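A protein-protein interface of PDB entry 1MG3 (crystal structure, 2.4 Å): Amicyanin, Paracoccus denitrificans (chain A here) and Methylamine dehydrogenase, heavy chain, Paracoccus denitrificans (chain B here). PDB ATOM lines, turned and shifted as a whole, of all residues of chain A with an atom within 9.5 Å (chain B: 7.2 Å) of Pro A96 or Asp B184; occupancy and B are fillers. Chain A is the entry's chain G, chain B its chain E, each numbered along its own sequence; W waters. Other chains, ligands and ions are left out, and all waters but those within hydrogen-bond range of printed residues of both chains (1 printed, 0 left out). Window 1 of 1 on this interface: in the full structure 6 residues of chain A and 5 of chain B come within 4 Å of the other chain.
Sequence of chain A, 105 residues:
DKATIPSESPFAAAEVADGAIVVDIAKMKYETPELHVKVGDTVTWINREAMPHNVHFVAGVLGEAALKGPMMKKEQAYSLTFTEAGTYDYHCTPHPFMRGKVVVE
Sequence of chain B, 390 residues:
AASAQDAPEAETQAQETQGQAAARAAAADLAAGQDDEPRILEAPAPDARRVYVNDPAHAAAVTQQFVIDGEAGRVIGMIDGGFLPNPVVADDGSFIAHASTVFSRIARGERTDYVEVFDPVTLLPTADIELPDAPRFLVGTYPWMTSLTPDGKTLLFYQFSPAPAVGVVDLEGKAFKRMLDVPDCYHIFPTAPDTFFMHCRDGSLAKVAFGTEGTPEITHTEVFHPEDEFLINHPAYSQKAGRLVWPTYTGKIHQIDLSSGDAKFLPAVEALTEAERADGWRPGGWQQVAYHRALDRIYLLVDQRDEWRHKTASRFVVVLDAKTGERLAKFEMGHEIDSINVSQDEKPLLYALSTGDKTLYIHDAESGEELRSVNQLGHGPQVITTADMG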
ATOM      1  N   MET A  28       2.291  15.549  19.992  1.00  0.00           N
ATOM      2  CA  MET A  28       1.810  16.542  19.041  1.00  0.00           C
ATOM      3  C   MET A  28       1.239  17.768  19.725  1.00  0.00           C
ATOM      4  O   MET A  28       0.171  18.251  19.351  1.00  0.00           O
ATOM      5  CB  MET A  28       0.734  15.941  18.126  1.00  0.00           C
ATOM      6  CG  MET A  28       1.211  14.792  17.238  1.00  0.00           C
ATOM      7  SD  MET A  28       2.596  15.227  16.165  1.00  0.00           S
ATOM      8  CE  MET A  28       1.741  16.029  14.807  1.00  0.00           C
ATOM      9  N   TYR A  30       2.416  21.397  22.527  1.00  0.00           N
ATOM     10  CA  TYR A  30       3.302  22.139  23.405  1.00  0.00           C
ATOM     11  C   TYR A  30       2.652  21.976  24.781  1.00  0.00           C
ATOM     12  O   TYR A  30       1.563  22.507  25.029  1.00  0.00           O
ATOM     13  CB  TYR A  30       3.330  23.612  22.999  1.00  0.00           C
ATOM     14  CG  TYR A  30       3.925  23.865  21.634  1.00  0.00           C
ATOM     15  CD1 TYR A  30       5.283  23.662  21.398  1.00  0.00           C
ATOM     16  CD2 TYR A  30       3.132  24.292  20.574  1.00  0.00           C
ATOM     17  CE1 TYR A  30       5.841  23.877  20.140  1.00  0.00           C
ATOM     18  CE2 TYR A  30       3.681  24.509  19.308  1.00  0.00           C
ATOM     19  CZ  TYR A  30       5.036  24.299  19.100  1.00  0.00           C
ATOM     20  OH  TYR A  30       5.589  24.510  17.856  1.00  0.00           O
ATOM     21  N   HIS A  53       9.729  18.738  15.704  1.00  0.00           N
ATOM     22  CA  HIS A  53       8.939  19.934  16.002  1.00  0.00           C
ATOM     23  C   HIS A  53       9.856  21.148  16.120  1.00  0.00           C
ATOM     24  O   HIS A  53      11.011  21.040  16.555  1.00  0.00           O
ATOM     25  CB  HIS A  53       8.189  19.791  17.339  1.00  0.00           C
ATOM     26  CG  HIS A  53       7.157  18.704  17.363  1.00  0.00           C
ATOM     27  ND1 HIS A  53       5.868  18.849  16.898  1.00  0.00           N
ATOM     28  CD2 HIS A  53       7.244  17.428  17.813  1.00  0.00           C
ATOM     29  CE1 HIS A  53       5.226  17.679  17.073  1.00  0.00           C
ATOM     30  NE2 HIS A  53       6.020  16.782  17.626  1.00  0.00           N
ATOM     31  N   ASN A  54       9.327  22.306  15.751  1.00  0.00           N
ATOM     32  CA  ASN A  54      10.067  23.556  15.849  1.00  0.00           C
ATOM     33  C   ASN A  54       9.072  24.585  16.378  1.00  0.00           C
ATOM     34  O   ASN A  54       7.921  24.267  16.672  1.00  0.00           O
ATOM     35  CB  ASN A  54      10.572  23.991  14.463  1.00  0.00           C
ATOM     36  CG  ASN A  54       9.456  24.562  13.575  1.00  0.00           C
ATOM     37  OD1 ASN A  54       8.305  24.129  13.648  1.00  0.00           O
ATOM     38  ND2 ASN A  54       9.804  25.528  12.727  1.00  0.00           N
ATOM     39  N   HIS A  56       7.573  28.443  15.445  1.00  0.00           N
ATOM     40  CA  HIS A  56       7.532  29.359  14.314  1.00  0.00           C
ATOM     41  C   HIS A  56       6.680  30.568  14.653  1.00  0.00           C
ATOM     42  O   HIS A  56       5.495  30.429  14.956  1.00  0.00           O
ATOM     43  CB  HIS A  56       6.968  28.584  13.107  1.00  0.00           C
ATOM     44  CG  HIS A  56       6.833  29.372  11.837  1.00  0.00           C
ATOM     45  ND1 HIS A  56       6.527  28.770  10.634  1.00  0.00           N
ATOM     46  CD2 HIS A  56       6.916  30.700  11.581  1.00  0.00           C
ATOM     47  CE1 HIS A  56       6.426  29.691   9.693  1.00  0.00           C
ATOM     48  NE2 HIS A  56       6.658  30.870  10.240  1.00  0.00           N
ATOM     49  N   MET A  71      13.996  22.686  13.221  1.00  0.00           N
ATOM     50  CA  MET A  71      13.317  21.493  13.719  1.00  0.00           C
ATOM     51  C   MET A  71      14.139  20.819  14.803  1.00  0.00           C
ATOM     52  O   MET A  71      15.338  20.636  14.656  1.00  0.00           O
ATOM     53  CB  MET A  71      13.097  20.486  12.586  1.00  0.00           C
ATOM     54  CG  MET A  71      12.076  20.898  11.562  1.00  0.00           C
ATOM     55  SD  MET A  71      10.503  21.179  12.352  1.00  0.00           S
ATOM     56  CE  MET A  71       9.787  22.297  11.192  1.00  0.00           C
ATOM     57  N   TYR A  90       2.806  31.450  18.449  1.00  0.00           N
ATOM     58  CA  TYR A  90       3.615  30.628  17.571  1.00  0.00           C
ATOM     59  C   TYR A  90       2.904  29.355  17.205  1.00  0.00           C
ATOM     60  O   TYR A  90       1.833  29.049  17.730  1.00  0.00           O
ATOM     61  CB  TYR A  90       4.967  30.274  18.204  1.00  0.00           C
ATOM     62  CG  TYR A  90       4.914  29.496  19.503  1.00  0.00           C
ATOM     63  CD1 TYR A  90       4.842  30.161  20.727  1.00  0.00           C
ATOM     64  CD2 TYR A  90       5.024  28.101  19.514  1.00  0.00           C
ATOM     65  CE1 TYR A  90       4.894  29.465  21.932  1.00  0.00           C
ATOM     66  CE2 TYR A  90       5.077  27.388  20.723  1.00  0.00           C
ATOM     67  CZ  TYR A  90       5.018  28.084  21.927  1.00  0.00           C
ATOM     68  OH  TYR A  90       5.122  27.420  23.131  1.00  0.00           O
ATOM     69  N   HIS A  91       3.508  28.618  16.286  1.00  0.00           N
ATOM     70  CA  HIS A  91       2.954  27.360  15.855  1.00  0.00           C
ATOM     71  C   HIS A  91       4.116  26.515  15.374  1.00  0.00           C
ATOM     72  O   HIS A  91       5.262  26.977  15.337  1.00  0.00           O
ATOM     73  CB  HIS A  91       1.948  27.564  14.718  1.00  0.00           C
ATOM     74  CG  HIS A  91       2.574  27.962  13.420  1.00  0.00           C
ATOM     75  ND1 HIS A  91       3.007  29.244  13.163  1.00  0.00           N
ATOM     76  CD2 HIS A  91       2.860  27.238  12.312  1.00  0.00           C
ATOM     77  CE1 HIS A  91       3.532  29.294  11.950  1.00  0.00           C
ATOM     78  NE2 HIS A  91       3.456  28.089  11.413  1.00  0.00           N
ATOM     79  N   CYS A  92       3.812  25.272  15.026  1.00  0.00           N
ATOM     80  CA  CYS A  92       4.813  24.349  14.538  1.00  0.00           C
ATOM     81  C   CYS A  92       4.690  24.439  13.024  1.00  0.00           C
ATOM     82  O   CYS A  92       3.596  24.286  12.484  1.00  0.00           O
ATOM     83  CB  CYS A  92       4.497  22.935  15.031  1.00  0.00           C
ATOM     84  SG  CYS A  92       5.853  21.776  14.821  1.00  0.00           S
ATOM     85  N   THR A  93       5.800  24.694  12.343  1.00  0.00           N
ATOM     86  CA  THR A  93       5.783  24.844  10.899  1.00  0.00           C
ATOM     87  C   THR A  93       5.054  23.744  10.128  1.00  0.00           C
ATOM     88  O   THR A  93       4.116  24.035   9.396  1.00  0.00           O
ATOM     89  CB  THR A  93       7.214  25.034  10.352  1.00  0.00           C
ATOM     90  OG1 THR A  93       7.785  26.209  10.938  1.00  0.00           O
ATOM     91  CG2 THR A  93       7.200  25.221   8.856  1.00  0.00           C
ATOM     92  N   PRO A  94       5.447  22.470  10.287  1.00  0.00           N
ATOM     93  CA  PRO A  94       4.738  21.426   9.538  1.00  0.00           C
ATOM     94  C   PRO A  94       3.413  20.995  10.157  1.00  0.00           C
ATOM     95  O   PRO A  94       2.631  20.284   9.529  1.00  0.00           O
ATOM     96  CB  PRO A  94       5.748  20.292   9.501  1.00  0.00           C
ATOM     97  CG  PRO A  94       6.382  20.407  10.850  1.00  0.00           C
ATOM     98  CD  PRO A  94       6.606  21.902  11.000  1.00  0.00           C
ATOM     99  N   HIS A  95       3.159  21.424  11.389  1.00  0.00           N
ATOM    100  CA  HIS A  95       1.927  21.061  12.090  1.00  0.00           C
ATOM    101  C   HIS A  95       1.205  22.321  12.594  1.00  0.00           C
ATOM    102  O   HIS A  95       1.126  22.573  13.799  1.00  0.00           O
ATOM    103  CB  HIS A  95       2.264  20.124  13.258  1.00  0.00           C
ATOM    104  CG  HIS A  95       3.166  18.985  12.876  1.00  0.00           C
ATOM    105  ND1 HIS A  95       4.236  18.559  13.634  1.00  0.00           N
ATOM    106  CD2 HIS A  95       3.156  18.188  11.777  1.00  0.00           C
ATOM    107  CE1 HIS A  95       4.829  17.549  12.987  1.00  0.00           C
ATOM    108  NE2 HIS A  95       4.211  17.286  11.853  1.00  0.00           N
ATOM    109  N   PRO A  96       0.644  23.116  11.661  1.00  0.00           N
ATOM    110  CA  PRO A  96      -0.073  24.359  11.958  1.00  0.00           C
ATOM    111  C   PRO A  96      -1.131  24.241  13.048  1.00  0.00           C
ATOM    112  O   PRO A  96      -1.512  25.241  13.649  1.00  0.00           O
ATOM    113  CB  PRO A  96      -0.674  24.746  10.606  1.00  0.00           C
ATOM    114  CG  PRO A  96       0.312  24.199   9.632  1.00  0.00           C
ATOM    115  CD  PRO A  96       0.600  22.830  10.215  1.00  0.00           C
ATOM    116  N   PHE A  97      -1.614  23.030  13.303  1.00  0.00           N
ATOM    117  CA  PHE A  97      -2.617  22.855  14.344  1.00  0.00           C
ATOM    118  C   PHE A  97      -1.992  22.938  15.729  1.00  0.00           C
ATOM    119  O   PHE A  97      -2.699  23.020  16.732  1.00  0.00           O
ATOM    120  CB  PHE A  97      -3.355  21.523  14.187  1.00  0.00           C
ATOM    121  CG  PHE A  97      -2.456  20.339  14.049  1.00  0.00           C
ATOM    122  CD1 PHE A  97      -1.865  20.043  12.827  1.00  0.00           C
ATOM    123  CD2 PHE A  97      -2.197  19.518  15.139  1.00  0.00           C
ATOM    124  CE1 PHE A  97      -1.025  18.944  12.686  1.00  0.00           C
ATOM    125  CE2 PHE A  97      -1.355  18.412  15.013  1.00  0.00           C
ATOM    126  CZ  PHE A  97      -0.766  18.125  13.777  1.00  0.00           C
ATOM    127  N   MET A  98      -0.664  22.912  15.786  1.00  0.00           N
ATOM    128  CA  MET A  98       0.041  23.019  17.060  1.00  0.00           C
ATOM    129  C   MET A  98       0.318  24.478  17.335  1.00  0.00           C
ATOM    130  O   MET A  98       1.048  25.119  16.592  1.00  0.00           O
ATOM    131  CB  MET A  98       1.368  22.266  17.014  1.00  0.00           C
ATOM    132  CG  MET A  98       1.243  20.781  17.248  1.00  0.00           C
ATOM    133  SD  MET A  98       2.837  19.995  17.054  1.00  0.00           S
ATOM    134  CE  MET A  98       3.529  20.233  18.707  1.00  0.00           C
ATOM    135  N   ARG A  99      -0.256  25.009  18.400  1.00  0.00           N
ATOM    136  CA  ARG A  99      -0.040  26.408  18.708  1.00  0.00           C
ATOM    137  C   ARG A  99       0.315  26.671  20.156  1.00  0.00           C
ATOM    138  O   ARG A  99       0.079  25.839  21.028  1.00  0.00           O
ATOM    139  CB  ARG A  99      -1.279  27.214  18.314  1.00  0.00           C
ATOM    140  CG  ARG A  99      -1.340  27.530  16.824  1.00  0.00           C
ATOM    141  CD  ARG A  99      -2.674  28.122  16.411  1.00  0.00           C
ATOM    142  NE  ARG A  99      -3.728  27.115  16.357  1.00  0.00           N
ATOM    143  CZ  ARG A  99      -4.268  26.648  15.234  1.00  0.00           C
ATOM    144  NH1 ARG A  99      -5.224  25.732  15.298  1.00  0.00           N
ATOM    145  NH2 ARG A  99      -3.866  27.096  14.051  1.00  0.00           N
ATOM    146  N   GLY A 100       0.902  27.837  20.391  1.00  0.00           N
ATOM    147  CA  GLY A 100       1.291  28.241  21.727  1.00  0.00           C
ATOM    148  C   GLY A 100       1.611  29.722  21.738  1.00  0.00           C
ATOM    149  O   GLY A 100       1.756  30.346  20.686  1.00  0.00           O
ATOM    150  N   TYR B 158      -7.540  27.469  -0.621  1.00  0.00           N
ATOM    151  CA  TYR B 158      -7.018  27.179   0.704  1.00  0.00           C
ATOM    152  C   TYR B 158      -5.576  27.604   0.904  1.00  0.00           C
ATOM    153  O   TYR B 158      -4.805  27.697  -0.047  1.00  0.00           O
ATOM    154  CB  TYR B 158      -7.131  25.680   0.976  1.00  0.00           C
ATOM    155  CG  TYR B 158      -6.679  25.264   2.361  1.00  0.00           C
ATOM    156  CD1 TYR B 158      -7.444  25.577   3.487  1.00  0.00           C
ATOM    157  CD2 TYR B 158      -5.492  24.548   2.546  1.00  0.00           C
ATOM    158  CE1 TYR B 158      -7.043  25.185   4.766  1.00  0.00           C
ATOM    159  CE2 TYR B 158      -5.076  24.154   3.826  1.00  0.00           C
ATOM    160  CZ  TYR B 158      -5.860  24.478   4.929  1.00  0.00           C
ATOM    161  OH  TYR B 158      -5.467  24.109   6.194  1.00  0.00           O
ATOM    162  N   PHE B 160      -2.408  26.683   3.685  1.00  0.00           N
ATOM    163  CA  PHE B 160      -1.980  25.798   4.763  1.00  0.00           C
ATOM    164  C   PHE B 160      -1.051  26.472   5.775  1.00  0.00           C
ATOM    165  O   PHE B 160      -1.296  26.428   6.983  1.00  0.00           O
ATOM    166  CB  PHE B 160      -1.288  24.572   4.156  1.00  0.00           C
ATOM    167  CG  PHE B 160      -0.740  23.607   5.170  1.00  0.00           C
ATOM    168  CD1 PHE B 160      -1.585  22.766   5.885  1.00  0.00           C
ATOM    169  CD2 PHE B 160       0.621  23.540   5.410  1.00  0.00           C
ATOM    170  CE1 PHE B 160      -1.076  21.875   6.821  1.00  0.00           C
ATOM    171  CE2 PHE B 160       1.141  22.651   6.343  1.00  0.00           C
ATOM    172  CZ  PHE B 160       0.291  21.818   7.050  1.00  0.00           C
ATOM    173  N   SER B 161       0.017  27.093   5.282  1.00  0.00           N
ATOM    174  CA  SER B 161       0.985  27.750   6.151  1.00  0.00           C
ATOM    175  C   SER B 161       0.951  29.252   5.907  1.00  0.00           C
ATOM    176  O   SER B 161       0.620  29.694   4.810  1.00  0.00           O
ATOM    177  CB  SER B 161       2.381  27.195   5.864  1.00  0.00           C
ATOM    178  OG  SER B 161       3.310  27.619   6.841  1.00  0.00           O
ATOM    179  N   PRO B 162       1.303  30.065   6.921  1.00  0.00           N
ATOM    180  CA  PRO B 162       1.729  29.700   8.277  1.00  0.00           C
ATOM    181  C   PRO B 162       0.566  29.275   9.170  1.00  0.00           C
ATOM    182  O   PRO B 162       0.748  28.960  10.352  1.00  0.00           O
ATOM    183  CB  PRO B 162       2.399  30.977   8.769  1.00  0.00           C
ATOM    184  CG  PRO B 162       1.540  32.042   8.134  1.00  0.00           C
ATOM    185  CD  PRO B 162       1.355  31.526   6.730  1.00  0.00           C
ATOM    186  N   ALA B 163      -0.631  29.277   8.597  1.00  0.00           N
ATOM    187  CA  ALA B 163      -1.824  28.884   9.329  1.00  0.00           C
ATOM    188  C   ALA B 163      -3.003  28.704   8.371  1.00  0.00           C
ATOM    189  O   ALA B 163      -3.020  29.276   7.277  1.00  0.00           O
ATOM    190  CB  ALA B 163      -2.147  29.926  10.382  1.00  0.00           C
ATOM    191  N   PRO B 164      -4.005  27.902   8.771  1.00  0.00           N
ATOM    192  CA  PRO B 164      -5.178  27.667   7.917  1.00  0.00           C
ATOM    193  C   PRO B 164      -5.910  28.961   7.589  1.00  0.00           C
ATOM    194  O   PRO B 164      -6.072  29.832   8.445  1.00  0.00           O
ATOM    195  CB  PRO B 164      -6.027  26.718   8.753  1.00  0.00           C
ATOM    196  CG  PRO B 164      -5.713  27.151  10.152  1.00  0.00           C
ATOM    197  CD  PRO B 164      -4.213  27.337  10.116  1.00  0.00           C
ATOM    198  N   VAL B 182      -9.450  30.597   9.411  1.00  0.00           N
ATOM    199  CA  VAL B 182     -10.311  29.442   9.611  1.00  0.00           C
ATOM    200  C   VAL B 182      -9.746  28.457  10.644  1.00  0.00           C
ATOM    201  O   VAL B 182      -8.570  28.508  10.979  1.00  0.00           O
ATOM    202  CB  VAL B 182     -10.495  28.742   8.253  1.00  0.00           C
ATOM    203  CG1 VAL B 182     -11.367  27.528   8.385  1.00  0.00           C
ATOM    204  CG2 VAL B 182     -11.101  29.716   7.271  1.00  0.00           C
ATOM    205  N   PRO B 183     -10.589  27.566  11.188  1.00  0.00           N
ATOM    206  CA  PRO B 183     -10.025  26.625  12.165  1.00  0.00           C
ATOM    207  C   PRO B 183      -9.096  25.671  11.422  1.00  0.00           C
ATOM    208  O   PRO B 183      -8.914  25.817  10.218  1.00  0.00           O
ATOM    209  CB  PRO B 183     -11.265  25.910  12.706  1.00  0.00           C
ATOM    210  CG  PRO B 183     -12.339  26.938  12.575  1.00  0.00           C
ATOM    211  CD  PRO B 183     -12.061  27.541  11.220  1.00  0.00           C
ATOM    212  N   ASP B 184      -8.515  24.696  12.125  1.00  0.00           N
ATOM    213  CA  ASP B 184      -7.627  23.720  11.485  1.00  0.00           C
ATOM    214  C   ASP B 184      -8.466  22.792  10.633  1.00  0.00           C
ATOM    215  O   ASP B 184      -8.602  21.618  10.939  1.00  0.00           O
ATOM    216  CB  ASP B 184      -6.871  22.879  12.519  1.00  0.00           C
ATOM    217  CG  ASP B 184      -5.963  23.708  13.392  1.00  0.00           C
ATOM    218  OD1 ASP B 184      -5.297  24.628  12.862  1.00  0.00           O
ATOM    219  OD2 ASP B 184      -5.912  23.430  14.611  1.00  0.00           O
ATOM    220  N   CYS B 185      -9.016  23.331   9.554  1.00  0.00           N
ATOM    221  CA  CYS B 185      -9.864  22.558   8.665  1.00  0.00           C
ATOM    222  C   CYS B 185      -9.303  22.567   7.246  1.00  0.00           C
ATOM    223  O   CYS B 185      -8.489  23.429   6.887  1.00  0.00           O
ATOM    224  CB  CYS B 185     -11.277  23.133   8.709  1.00  0.00           C
ATOM    225  SG  CYS B 185     -11.815  23.461  10.410  1.00  0.00           S
ATOM    226  N   TYR B 186      -9.737  21.605   6.440  1.00  0.00           N
ATOM    227  CA  TYR B 186      -9.232  21.481   5.087  1.00  0.00           C
ATOM    228  C   TYR B 186     -10.336  21.299   4.047  1.00  0.00           C
ATOM    229  O   TYR B 186     -11.421  20.824   4.361  1.00  0.00           O
ATOM    230  CB  TYR B 186      -8.234  20.312   5.045  1.00  0.00           C
ATOM    231  CG  TYR B 186      -7.229  20.362   6.187  1.00  0.00           C
ATOM    232  CD1 TYR B 186      -7.588  19.969   7.474  1.00  0.00           C
ATOM    233  CD2 TYR B 186      -5.948  20.883   5.996  1.00  0.00           C
ATOM    234  CE1 TYR B 186      -6.705  20.103   8.546  1.00  0.00           C
ATOM    235  CE2 TYR B 186      -5.056  21.021   7.062  1.00  0.00           C
ATOM    236  CZ  TYR B 186      -5.447  20.631   8.333  1.00  0.00           C
ATOM    237  OH  TYR B 186      -4.597  20.803   9.402  1.00  0.00           O
ATOM    238  N   MET B 198     -16.009  23.081   5.376  1.00  0.00           N
ATOM    239  CA  MET B 198     -14.663  22.516   5.420  1.00  0.00           C
ATOM    240  C   MET B 198     -14.631  21.252   6.275  1.00  0.00           C
ATOM    241  O   MET B 198     -15.533  21.001   7.080  1.00  0.00           O
ATOM    242  CB  MET B 198     -13.670  23.525   6.005  1.00  0.00           C
ATOM    243  CG  MET B 198     -13.591  24.836   5.242  1.00  0.00           C
ATOM    244  SD  MET B 198     -12.307  25.930   5.877  1.00  0.00           S
ATOM    245  CE  MET B 198     -10.909  25.474   4.878  1.00  0.00           C
ATOM    246  N   HIS B 199     -13.595  20.448   6.086  1.00  0.00           N
ATOM    247  CA  HIS B 199     -13.427  19.239   6.873  1.00  0.00           C
ATOM    248  C   HIS B 199     -12.354  19.557   7.912  1.00  0.00           C
ATOM    249  O   HIS B 199     -11.275  20.030   7.557  1.00  0.00           O
ATOM    250  CB  HIS B 199     -12.957  18.088   6.003  1.00  0.00           C
ATOM    251  CG  HIS B 199     -12.749  16.825   6.767  1.00  0.00           C
ATOM    252  ND1 HIS B 199     -11.776  15.906   6.440  1.00  0.00           N
ATOM    253  CD2 HIS B 199     -13.401  16.321   7.839  1.00  0.00           C
ATOM    254  CE1 HIS B 199     -11.838  14.889   7.281  1.00  0.00           C
ATOM    255  NE2 HIS B 199     -12.817  15.114   8.139  1.00  0.00           N
ATOM    256  N   CYS B 200     -12.629  19.298   9.185  1.00  0.00           N
ATOM    257  CA  CYS B 200     -11.651  19.631  10.214  1.00  0.00           C
ATOM    258  C   CYS B 200     -10.908  18.444  10.801  1.00  0.00           C
ATOM    259  O   CYS B 200     -11.364  17.303  10.723  1.00  0.00           O
ATOM    260  CB  CYS B 200     -12.324  20.404  11.343  1.00  0.00           C
ATOM    261  SG  CYS B 200     -13.495  21.616  10.752  1.00  0.00           S
ATOM    262  N   ARG B 201      -9.761  18.737  11.403  1.00  0.00           N
ATOM    263  CA  ARG B 201      -8.919  17.720  12.000  1.00  0.00           C
ATOM    264  C   ARG B 201      -9.644  16.898  13.055  1.00  0.00           C
ATOM    265  O   ARG B 201      -9.432  15.693  13.142  1.00  0.00           O
ATOM    266  CB  ARG B 201      -7.678  18.369  12.616  1.00  0.00           C
ATOM    267  CG  ARG B 201      -6.650  17.378  13.146  1.00  0.00           C
ATOM    268  CD  ARG B 201      -5.586  18.061  13.996  1.00  0.00           C
ATOM    269  NE  ARG B 201      -4.697  17.082  14.614  1.00  0.00           N
ATOM    270  CZ  ARG B 201      -3.745  16.426  13.960  1.00  0.00           C
ATOM    271  NH1 ARG B 201      -2.987  15.542  14.600  1.00  0.00           N
ATOM    272  NH2 ARG B 201      -3.533  16.669  12.670  1.00  0.00           N
ATOM    273  N   ASP B 202     -10.500  17.530  13.851  1.00  0.00           N
ATOM    274  CA  ASP B 202     -11.207  16.803  14.904  1.00  0.00           C
ATOM    275  C   ASP B 202     -12.294  15.861  14.404  1.00  0.00           C
ATOM    276  O   ASP B 202     -12.922  15.165  15.197  1.00  0.00           O
ATOM    277  CB  ASP B 202     -11.827  17.768  15.914  1.00  0.00           C
ATOM    278  CG  ASP B 202     -12.828  18.701  15.282  1.00  0.00           C
ATOM    279  OD1 ASP B 202     -13.414  18.322  14.243  1.00  0.00           O
ATOM    280  OD2 ASP B 202     -13.037  19.806  15.829  1.00  0.00           O
ATOM    281  N   ALA B 206     -16.789  22.186   9.213  1.00  0.00           N
ATOM    282  CA  ALA B 206     -16.811  23.586   9.600  1.00  0.00           C
ATOM    283  C   ALA B 206     -17.643  24.409   8.630  1.00  0.00           C
ATOM    284  O   ALA B 206     -17.475  24.317   7.413  1.00  0.00           O
ATOM    285  CB  ALA B 206     -15.380  24.133   9.666  1.00  0.00           C
ATOM    286  N   HIS B 220     -19.134  24.566  13.958  1.00  0.00           N
ATOM    287  CA  HIS B 220     -18.786  23.175  13.672  1.00  0.00           C
ATOM    288  C   HIS B 220     -19.990  22.265  13.767  1.00  0.00           C
ATOM    289  O   HIS B 220     -20.905  22.524  14.534  1.00  0.00           O
ATOM    290  CB  HIS B 220     -17.744  22.674  14.665  1.00  0.00           C
ATOM    291  CG  HIS B 220     -16.404  23.308  14.510  1.00  0.00           C
ATOM    292  ND1 HIS B 220     -15.354  22.681  13.871  1.00  0.00           N
ATOM    293  CD2 HIS B 220     -15.942  24.526  14.885  1.00  0.00           C
ATOM    294  CE1 HIS B 220     -14.305  23.486  13.859  1.00  0.00           C
ATOM    295  NE2 HIS B 220     -14.635  24.612  14.466  1.00  0.00           N
HETATM  296  O   HOH W   1       4.032  26.824   9.096  1.00  0.00           O
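The backbone carbonyl oxygen (O) of Pro B162 lies within hydrogen-bond range of a ring nitrogen (NE2) of His A91 (3.0 Å).
OD2 of Asp B184 is in salt-bridge range of NH1 of Arg A99.
The backbone NH (N) of His A56 sits at hydrogen-bond distance from the backbone carbonyl oxygen (O) of His A91 (2.7 Å).
NH2 of Arg A99 sits at hydrogen-bond distance from O of Pro A96 (3.0 Å).
The backbone carbonyl oxygen (O) of Asp B184 is in hydrogen-bond range of the backbone NH (N) of Arg B201.
Among the printed residues, pairs that only touch across the chains: Phe A97 with Asp B184 (3.2 Å), Phe A97 with Arg B201 (3.3 Å), Pro A96 with Phe B160 (3.3 Å), Pro A94 with Phe B160 (3.7 Å), Pro A96 with Asp B184 (3.9 Å) and Arg A99 with Pro B164 (3.96 Å).
Pro A96 touches two residues of chain B.
Asp B184 touches just these residues of chain A: Pro A96, Phe A97 and Arg A99.
No residue of chain A comes within 4 Å of Pro B183.
No residue of chain A comes within 4 Å of Cys B185.
Printed residues of chain A within 4 Å of Pro B162: His A91 (3.0 Å).
Of the printed residues of chain A, Phe B160 touches Pro A94 and Pro A96.
Cys A92 touches none of the printed residues of chain B.
The nearest residue of chain A that does not touch Asp B184 is Met A98 (5.4 Å).
Of the 17 printed residues of chain A, 5 touch a printed residue of chain B.
Printed residues of chain A that touch a printed residue of chain B: His A91, Pro A94, Pro A96, Phe A97 and Arg A99.
Of the 18 printed residues of chain B, 5 touch a printed residue of chain A.
Among the printed residues, 8 pairs touch across the chains.
Water W1 lies within hydrogen-bond range of OG of Ser B161 (2.5 Å), NE2 of His A91 (2.7 Å) and O of Thr A93 (2.8 Å).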
